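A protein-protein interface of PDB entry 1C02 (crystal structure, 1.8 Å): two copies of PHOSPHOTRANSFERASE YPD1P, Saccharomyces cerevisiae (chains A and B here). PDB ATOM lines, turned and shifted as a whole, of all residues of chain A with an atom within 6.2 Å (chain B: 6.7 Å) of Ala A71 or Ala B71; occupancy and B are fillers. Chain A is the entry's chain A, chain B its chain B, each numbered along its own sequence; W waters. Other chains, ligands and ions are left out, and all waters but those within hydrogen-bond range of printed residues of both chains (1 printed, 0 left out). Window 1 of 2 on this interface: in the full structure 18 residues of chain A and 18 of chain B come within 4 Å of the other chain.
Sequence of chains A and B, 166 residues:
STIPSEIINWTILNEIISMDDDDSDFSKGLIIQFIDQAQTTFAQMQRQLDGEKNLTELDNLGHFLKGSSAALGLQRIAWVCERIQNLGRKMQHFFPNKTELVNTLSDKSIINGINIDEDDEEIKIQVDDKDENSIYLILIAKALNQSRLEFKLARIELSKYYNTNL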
ATOM      1  N   ILE A  12     -16.936  -6.409 -24.786  1.00  0.00           N
ATOM      2  CA  ILE A  12     -16.255  -5.528 -23.840  1.00  0.00           C
ATOM      3  C   ILE A  12     -17.195  -4.431 -23.353  1.00  0.00           C
ATOM      4  O   ILE A  12     -17.372  -4.256 -22.148  1.00  0.00           O
ATOM      5  CB  ILE A  12     -14.995  -4.865 -24.449  1.00  0.00           C
ATOM      6  CG1 ILE A  12     -13.974  -5.932 -24.839  1.00  0.00           C
ATOM      7  CG2 ILE A  12     -14.368  -3.904 -23.452  1.00  0.00           C
ATOM      8  CD1 ILE A  12     -13.750  -6.969 -23.772  1.00  0.00           C
ATOM      9  N   LEU A  13     -17.856  -3.739 -24.280  1.00  0.00           N
ATOM     10  CA  LEU A  13     -18.688  -2.608 -23.890  1.00  0.00           C
ATOM     11  C   LEU A  13     -19.928  -3.025 -23.098  1.00  0.00           C
ATOM     12  O   LEU A  13     -20.360  -2.291 -22.211  1.00  0.00           O
ATOM     13  CB  LEU A  13     -19.103  -1.770 -25.100  1.00  0.00           C
ATOM     14  CG  LEU A  13     -19.704  -0.413 -24.707  1.00  0.00           C
ATOM     15  CD1 LEU A  13     -18.721   0.364 -23.850  1.00  0.00           C
ATOM     16  CD2 LEU A  13     -20.076   0.394 -25.949  1.00  0.00           C
ATOM     17  N   ILE A  16     -19.182  -2.999 -19.466  1.00  0.00           N
ATOM     18  CA  ILE A  16     -19.196  -1.646 -18.907  1.00  0.00           C
ATOM     19  C   ILE A  16     -20.646  -1.194 -18.730  1.00  0.00           C
ATOM     20  O   ILE A  16     -21.003  -0.622 -17.702  1.00  0.00           O
ATOM     21  CB  ILE A  16     -18.483  -0.629 -19.831  1.00  0.00           C
ATOM     22  CG1 ILE A  16     -17.058  -1.097 -20.172  1.00  0.00           C
ATOM     23  CG2 ILE A  16     -18.455   0.729 -19.170  1.00  0.00           C
ATOM     24  CD1 ILE A  16     -16.091  -1.096 -19.006  1.00  0.00           C
ATOM     25  N   LYS A  66      -4.221   4.187 -27.077  1.00  0.00           N
ATOM     26  CA  LYS A  66      -4.461   2.761 -27.289  1.00  0.00           C
ATOM     27  C   LYS A  66      -5.089   2.143 -26.036  1.00  0.00           C
ATOM     28  O   LYS A  66      -6.015   1.341 -26.128  1.00  0.00           O
ATOM     29  CB  LYS A  66      -3.154   2.023 -27.632  1.00  0.00           C
ATOM     30  CG  LYS A  66      -3.351   0.515 -27.801  1.00  0.00           C
ATOM     31  CD  LYS A  66      -2.113  -0.184 -28.322  1.00  0.00           C
ATOM     32  CE  LYS A  66      -1.042  -0.291 -27.274  1.00  0.00           C
ATOM     33  NZ  LYS A  66       0.178  -0.979 -27.802  1.00  0.00           N
ATOM     34  N   GLY A  67      -4.543   2.478 -24.875  1.00  0.00           N
ATOM     35  CA  GLY A  67      -5.062   1.940 -23.633  1.00  0.00           C
ATOM     36  C   GLY A  67      -6.490   2.385 -23.394  1.00  0.00           C
ATOM     37  O   GLY A  67      -7.345   1.567 -23.099  1.00  0.00           O
ATOM     38  N   SER A  68      -6.756   3.674 -23.576  1.00  0.00           N
ATOM     39  CA  SER A  68      -8.081   4.234 -23.336  1.00  0.00           C
ATOM     40  C   SER A  68      -9.112   3.630 -24.269  1.00  0.00           C
ATOM     41  O   SER A  68     -10.215   3.291 -23.842  1.00  0.00           O
ATOM     42  CB  SER A  68      -8.067   5.753 -23.532  1.00  0.00           C
ATOM     43  OG  SER A  68      -7.363   6.399 -22.493  1.00  0.00           O
ATOM     44  N   SER A  69      -8.781   3.570 -25.555  1.00  0.00           N
ATOM     45  CA  SER A  69      -9.706   3.041 -26.542  1.00  0.00           C
ATOM     46  C   SER A  69      -9.962   1.531 -26.439  1.00  0.00           C
ATOM     47  O   SER A  69     -11.096   1.090 -26.597  1.00  0.00           O
ATOM     48  CB  SER A  69      -9.250   3.420 -27.960  1.00  0.00           C
ATOM     49  OG  SER A  69      -7.925   2.998 -28.215  1.00  0.00           O
ATOM     50  N   ALA A  70      -8.945   0.751 -26.081  1.00  0.00           N
ATOM     51  CA  ALA A  70      -9.104  -0.701 -25.958  1.00  0.00           C
ATOM     52  C   ALA A  70     -10.037  -1.052 -24.803  1.00  0.00           C
ATOM     53  O   ALA A  70     -10.885  -1.940 -24.930  1.00  0.00           O
ATOM     54  CB  ALA A  70      -7.754  -1.360 -25.736  1.00  0.00           C
ATOM     55  N   ALA A  71      -9.883  -0.332 -23.692  1.00  0.00           N
ATOM     56  CA  ALA A  71     -10.668  -0.558 -22.474  1.00  0.00           C
ATOM     57  C   ALA A  71     -12.165  -0.344 -22.670  1.00  0.00           C
ATOM     58  O   ALA A  71     -12.967  -0.942 -21.965  1.00  0.00           O
ATOM     59  CB  ALA A  71     -10.163   0.346 -21.361  1.00  0.00           C
ATOM     60  N   LEU A  72     -12.532   0.515 -23.621  1.00  0.00           N
ATOM     61  CA  LEU A  72     -13.933   0.784 -23.927  1.00  0.00           C
ATOM     62  C   LEU A  72     -14.436  -0.028 -25.110  1.00  0.00           C
ATOM     63  O   LEU A  72     -15.562   0.145 -25.552  1.00  0.00           O
ATOM     64  CB  LEU A  72     -14.138   2.268 -24.213  1.00  0.00           C
ATOM     65  CG  LEU A  72     -13.950   3.162 -22.995  1.00  0.00           C
ATOM     66  CD1 LEU A  72     -13.965   4.628 -23.401  1.00  0.00           C
ATOM     67  CD2 LEU A  72     -15.049   2.849 -22.003  1.00  0.00           C
ATOM     68  N   GLY A  73     -13.584  -0.900 -25.636  1.00  0.00           N
ATOM     69  CA  GLY A  73     -13.998  -1.774 -26.717  1.00  0.00           C
ATOM     70  C   GLY A  73     -13.943  -1.134 -28.089  1.00  0.00           C
ATOM     71  O   GLY A  73     -14.486  -1.678 -29.045  1.00  0.00           O
ATOM     72  N   LEU A  74     -13.301   0.027 -28.192  1.00  0.00           N
ATOM     73  CA  LEU A  74     -13.176   0.715 -29.478  1.00  0.00           C
ATOM     74  C   LEU A  74     -11.912   0.218 -30.182  1.00  0.00           C
ATOM     75  O   LEU A  74     -10.894   0.896 -30.224  1.00  0.00           O
ATOM     76  CB  LEU A  74     -13.146   2.232 -29.261  1.00  0.00           C
ATOM     77  CG  LEU A  74     -14.307   2.765 -28.414  1.00  0.00           C
ATOM     78  CD1 LEU A  74     -14.132   4.237 -28.171  1.00  0.00           C
ATOM     79  CD2 LEU A  74     -15.616   2.521 -29.114  1.00  0.00           C
ATOM     80  N   ILE B  12     -12.881 -10.273 -20.464  1.00  0.00           N
ATOM     81  CA  ILE B  12     -12.457  -8.881 -20.569  1.00  0.00           C
ATOM     82  C   ILE B  12     -10.936  -8.750 -20.654  1.00  0.00           C
ATOM     83  O   ILE B  12     -10.416  -8.158 -21.596  1.00  0.00           O
ATOM     84  CB  ILE B  12     -12.968  -8.027 -19.382  1.00  0.00           C
ATOM     85  CG1 ILE B  12     -14.499  -8.048 -19.342  1.00  0.00           C
ATOM     86  CG2 ILE B  12     -12.441  -6.586 -19.493  1.00  0.00           C
ATOM     87  CD1 ILE B  12     -15.147  -7.534 -20.595  1.00  0.00           C
ATOM     88  N   LEU B  13     -10.222  -9.307 -19.678  1.00  0.00           N
ATOM     89  CA  LEU B  13      -8.770  -9.126 -19.601  1.00  0.00           C
ATOM     90  C   LEU B  13      -8.031  -9.746 -20.783  1.00  0.00           C
ATOM     91  O   LEU B  13      -7.032  -9.198 -21.244  1.00  0.00           O
ATOM     92  CB  LEU B  13      -8.216  -9.694 -18.285  1.00  0.00           C
ATOM     93  CG  LEU B  13      -6.771  -9.310 -17.925  1.00  0.00           C
ATOM     94  CD1 LEU B  13      -6.556  -7.797 -17.978  1.00  0.00           C
ATOM     95  CD2 LEU B  13      -6.455  -9.820 -16.526  1.00  0.00           C
ATOM     96  N   ILE B  16      -7.554  -7.372 -23.593  1.00  0.00           N
ATOM     97  CA  ILE B  16      -6.462  -6.444 -23.344  1.00  0.00           C
ATOM     98  C   ILE B  16      -5.127  -7.154 -23.605  1.00  0.00           C
ATOM     99  O   ILE B  16      -4.218  -6.575 -24.204  1.00  0.00           O
ATOM    100  CB  ILE B  16      -6.529  -5.920 -21.872  1.00  0.00           C
ATOM    101  CG1 ILE B  16      -7.835  -5.147 -21.652  1.00  0.00           C
ATOM    102  CG2 ILE B  16      -5.292  -5.088 -21.525  1.00  0.00           C
ATOM    103  CD1 ILE B  16      -7.744  -3.661 -21.928  1.00  0.00           C
ATOM    104  N   LEU B  30      -0.417  -1.640 -17.871  1.00  0.00           N
ATOM    105  CA  LEU B  30      -1.697  -1.128 -17.406  1.00  0.00           C
ATOM    106  C   LEU B  30      -2.004  -1.633 -15.996  1.00  0.00           C
ATOM    107  O   LEU B  30      -2.531  -0.895 -15.158  1.00  0.00           O
ATOM    108  CB  LEU B  30      -2.827  -1.553 -18.342  1.00  0.00           C
ATOM    109  CG  LEU B  30      -2.928  -1.001 -19.760  1.00  0.00           C
ATOM    110  CD1 LEU B  30      -4.250  -1.444 -20.353  1.00  0.00           C
ATOM    111  CD2 LEU B  30      -2.848   0.497 -19.743  1.00  0.00           C
ATOM    112  N   LYS B  66     -13.996   2.323  -9.667  1.00  0.00           N
ATOM    113  CA  LYS B  66     -14.940   1.428 -10.327  1.00  0.00           C
ATOM    114  C   LYS B  66     -14.693   1.421 -11.828  1.00  0.00           C
ATOM    115  O   LYS B  66     -14.684   0.363 -12.452  1.00  0.00           O
ATOM    116  CB  LYS B  66     -16.390   1.839 -10.052  1.00  0.00           C
ATOM    117  CG  LYS B  66     -17.403   0.909 -10.716  1.00  0.00           C
ATOM    118  CD  LYS B  66     -18.833   1.223 -10.323  1.00  0.00           C
ATOM    119  CE  LYS B  66     -19.356   2.415 -11.070  1.00  0.00           C
ATOM    120  NZ  LYS B  66     -20.730   2.752 -10.625  1.00  0.00           N
ATOM    121  N   GLY B  67     -14.417   2.595 -12.386  1.00  0.00           N
ATOM    122  CA  GLY B  67     -14.118   2.694 -13.806  1.00  0.00           C
ATOM    123  C   GLY B  67     -12.849   1.969 -14.207  1.00  0.00           C
ATOM    124  O   GLY B  67     -12.868   1.178 -15.146  1.00  0.00           O
ATOM    125  N   SER B  68     -11.779   2.164 -13.439  1.00  0.00           N
ATOM    126  CA  SER B  68     -10.475   1.552 -13.723  1.00  0.00           C
ATOM    127  C   SER B  68     -10.485   0.047 -13.522  1.00  0.00           C
ATOM    128  O   SER B  68      -9.865  -0.674 -14.278  1.00  0.00           O
ATOM    129  CB  SER B  68      -9.379   2.156 -12.833  1.00  0.00           C
ATOM    130  OG  SER B  68      -9.401   3.567 -12.884  1.00  0.00           O
ATOM    131  N   SER B  69     -11.120  -0.423 -12.452  1.00  0.00           N
ATOM    132  CA  SER B  69     -11.138  -1.855 -12.197  1.00  0.00           C
ATOM    133  C   SER B  69     -12.046  -2.628 -13.160  1.00  0.00           C
ATOM    134  O   SER B  69     -11.647  -3.668 -13.678  1.00  0.00           O
ATOM    135  CB  SER B  69     -11.508  -2.143 -10.738  1.00  0.00           C
ATOM    136  OG  SER B  69     -12.681  -1.470 -10.370  1.00  0.00           O
ATOM    137  N   ALA B  70     -13.195  -2.058 -13.516  1.00  0.00           N
ATOM    138  CA  ALA B  70     -14.112  -2.726 -14.440  1.00  0.00           C
ATOM    139  C   ALA B  70     -13.450  -2.938 -15.794  1.00  0.00           C
ATOM    140  O   ALA B  70     -13.507  -4.032 -16.340  1.00  0.00           O
ATOM    141  CB  ALA B  70     -15.372  -1.920 -14.615  1.00  0.00           C
ATOM    142  N   ALA B  71     -12.706  -1.934 -16.250  1.00  0.00           N
ATOM    143  CA  ALA B  71     -12.072  -1.948 -17.567  1.00  0.00           C
ATOM    144  C   ALA B  71     -10.993  -3.014 -17.712  1.00  0.00           C
ATOM    145  O   ALA B  71     -10.676  -3.434 -18.827  1.00  0.00           O
ATOM    146  CB  ALA B  71     -11.484  -0.594 -17.847  1.00  0.00           C
ATOM    147  N   LEU B  72     -10.407  -3.430 -16.592  1.00  0.00           N
ATOM    148  CA  LEU B  72      -9.408  -4.495 -16.584  1.00  0.00           C
ATOM    149  C   LEU B  72      -9.957  -5.841 -16.115  1.00  0.00           C
ATOM    150  O   LEU B  72      -9.199  -6.788 -15.897  1.00  0.00           O
ATOM    151  CB  LEU B  72      -8.243  -4.102 -15.700  1.00  0.00           C
ATOM    152  CG  LEU B  72      -7.449  -2.921 -16.241  1.00  0.00           C
ATOM    153  CD1 LEU B  72      -6.439  -2.491 -15.164  1.00  0.00           C
ATOM    154  CD2 LEU B  72      -6.743  -3.300 -17.558  1.00  0.00           C
ATOM    155  N   GLY B  73     -11.268  -5.912 -15.913  1.00  0.00           N
ATOM    156  CA  GLY B  73     -11.897  -7.190 -15.626  1.00  0.00           C
ATOM    157  C   GLY B  73     -11.833  -7.578 -14.162  1.00  0.00           C
ATOM    158  O   GLY B  73     -12.203  -8.692 -13.792  1.00  0.00           O
ATOM    159  N   LEU B  74     -11.429  -6.628 -13.321  1.00  0.00           N
ATOM    160  CA  LEU B  74     -11.352  -6.852 -11.885  1.00  0.00           C
ATOM    161  C   LEU B  74     -12.729  -6.571 -11.277  1.00  0.00           C
ATOM    162  O   LEU B  74     -12.948  -5.570 -10.602  1.00  0.00           O
ATOM    163  CB  LEU B  74     -10.248  -5.971 -11.274  1.00  0.00           C
ATOM    164  CG  LEU B  74      -8.883  -6.114 -11.974  1.00  0.00           C
ATOM    165  CD1 LEU B  74      -7.915  -5.105 -11.434  1.00  0.00           C
ATOM    166  CD2 LEU B  74      -8.326  -7.510 -11.756  1.00  0.00           C
ATOM    167  N   ALA B  78     -14.648  -3.806  -8.602  1.00  0.00           N
ATOM    168  CA  ALA B  78     -15.625  -2.891  -9.181  1.00  0.00           C
ATOM    169  C   ALA B  78     -16.953  -2.948  -8.426  1.00  0.00           C
ATOM    170  O   ALA B  78     -17.600  -1.930  -8.212  1.00  0.00           O
ATOM    171  CB  ALA B  78     -15.844  -3.221 -10.646  1.00  0.00           C
HETATM  172  O   HOH W   1     -12.533  -3.362 -20.787  1.00  0.00           O
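Ile A12 touches Ile B12 (CD1 to CD1, 3.5 Å).
CB of Ala A71 touches CB of Ala B71, 3.9 Å away.
Printed residues of chain B within 4 Å of Ile A12: Ile B12.
Ala A70 touches none of the printed residues of chain B.
Ala A71 touches just one residue of chain B: Ala B71.
Printed residues of chain A within 4 Å of Ile B12: Ile A12 (3.5 Å).
Ile B16 touches none of the printed residues of chain A.
Ala B71 touches just one residue of chain A: Ala A71 (3.9 Å).
Of the 12 printed residues of chain A, 2 touch a printed residue of chain B.
Hydrophobic or aromatic side chains of chain A that line the printed part of chain B: Ile A12 and Ala A71.
Along chain A the printed residues that touch a printed residue of chain B span positions 12 to 71.
Of the 14 printed residues of chain B, 2 touch a printed residue of chain A.
Hydrophobic or aromatic side chains of chain B that line the printed part of chain A: Ile B12 and Ala B71.
Among the printed residues, 2 pairs touch across the chains.
Among the printed residues, no Asp or Glu carboxylate lies within 4 Å of a Lys or Arg side-chain nitrogen of the other chain.
Ile A12 touches its own counterpart, Ile B12.
Ala A71 touches its own counterpart, Ala B71.
Of the 2 pairs that touch across the chains among the printed residues, 2 have their exchanged pair printed and touching as well.
Water W1 bridges O of Ala B71 (2.7 Å) and O of Ala A71 (2.7 Å).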
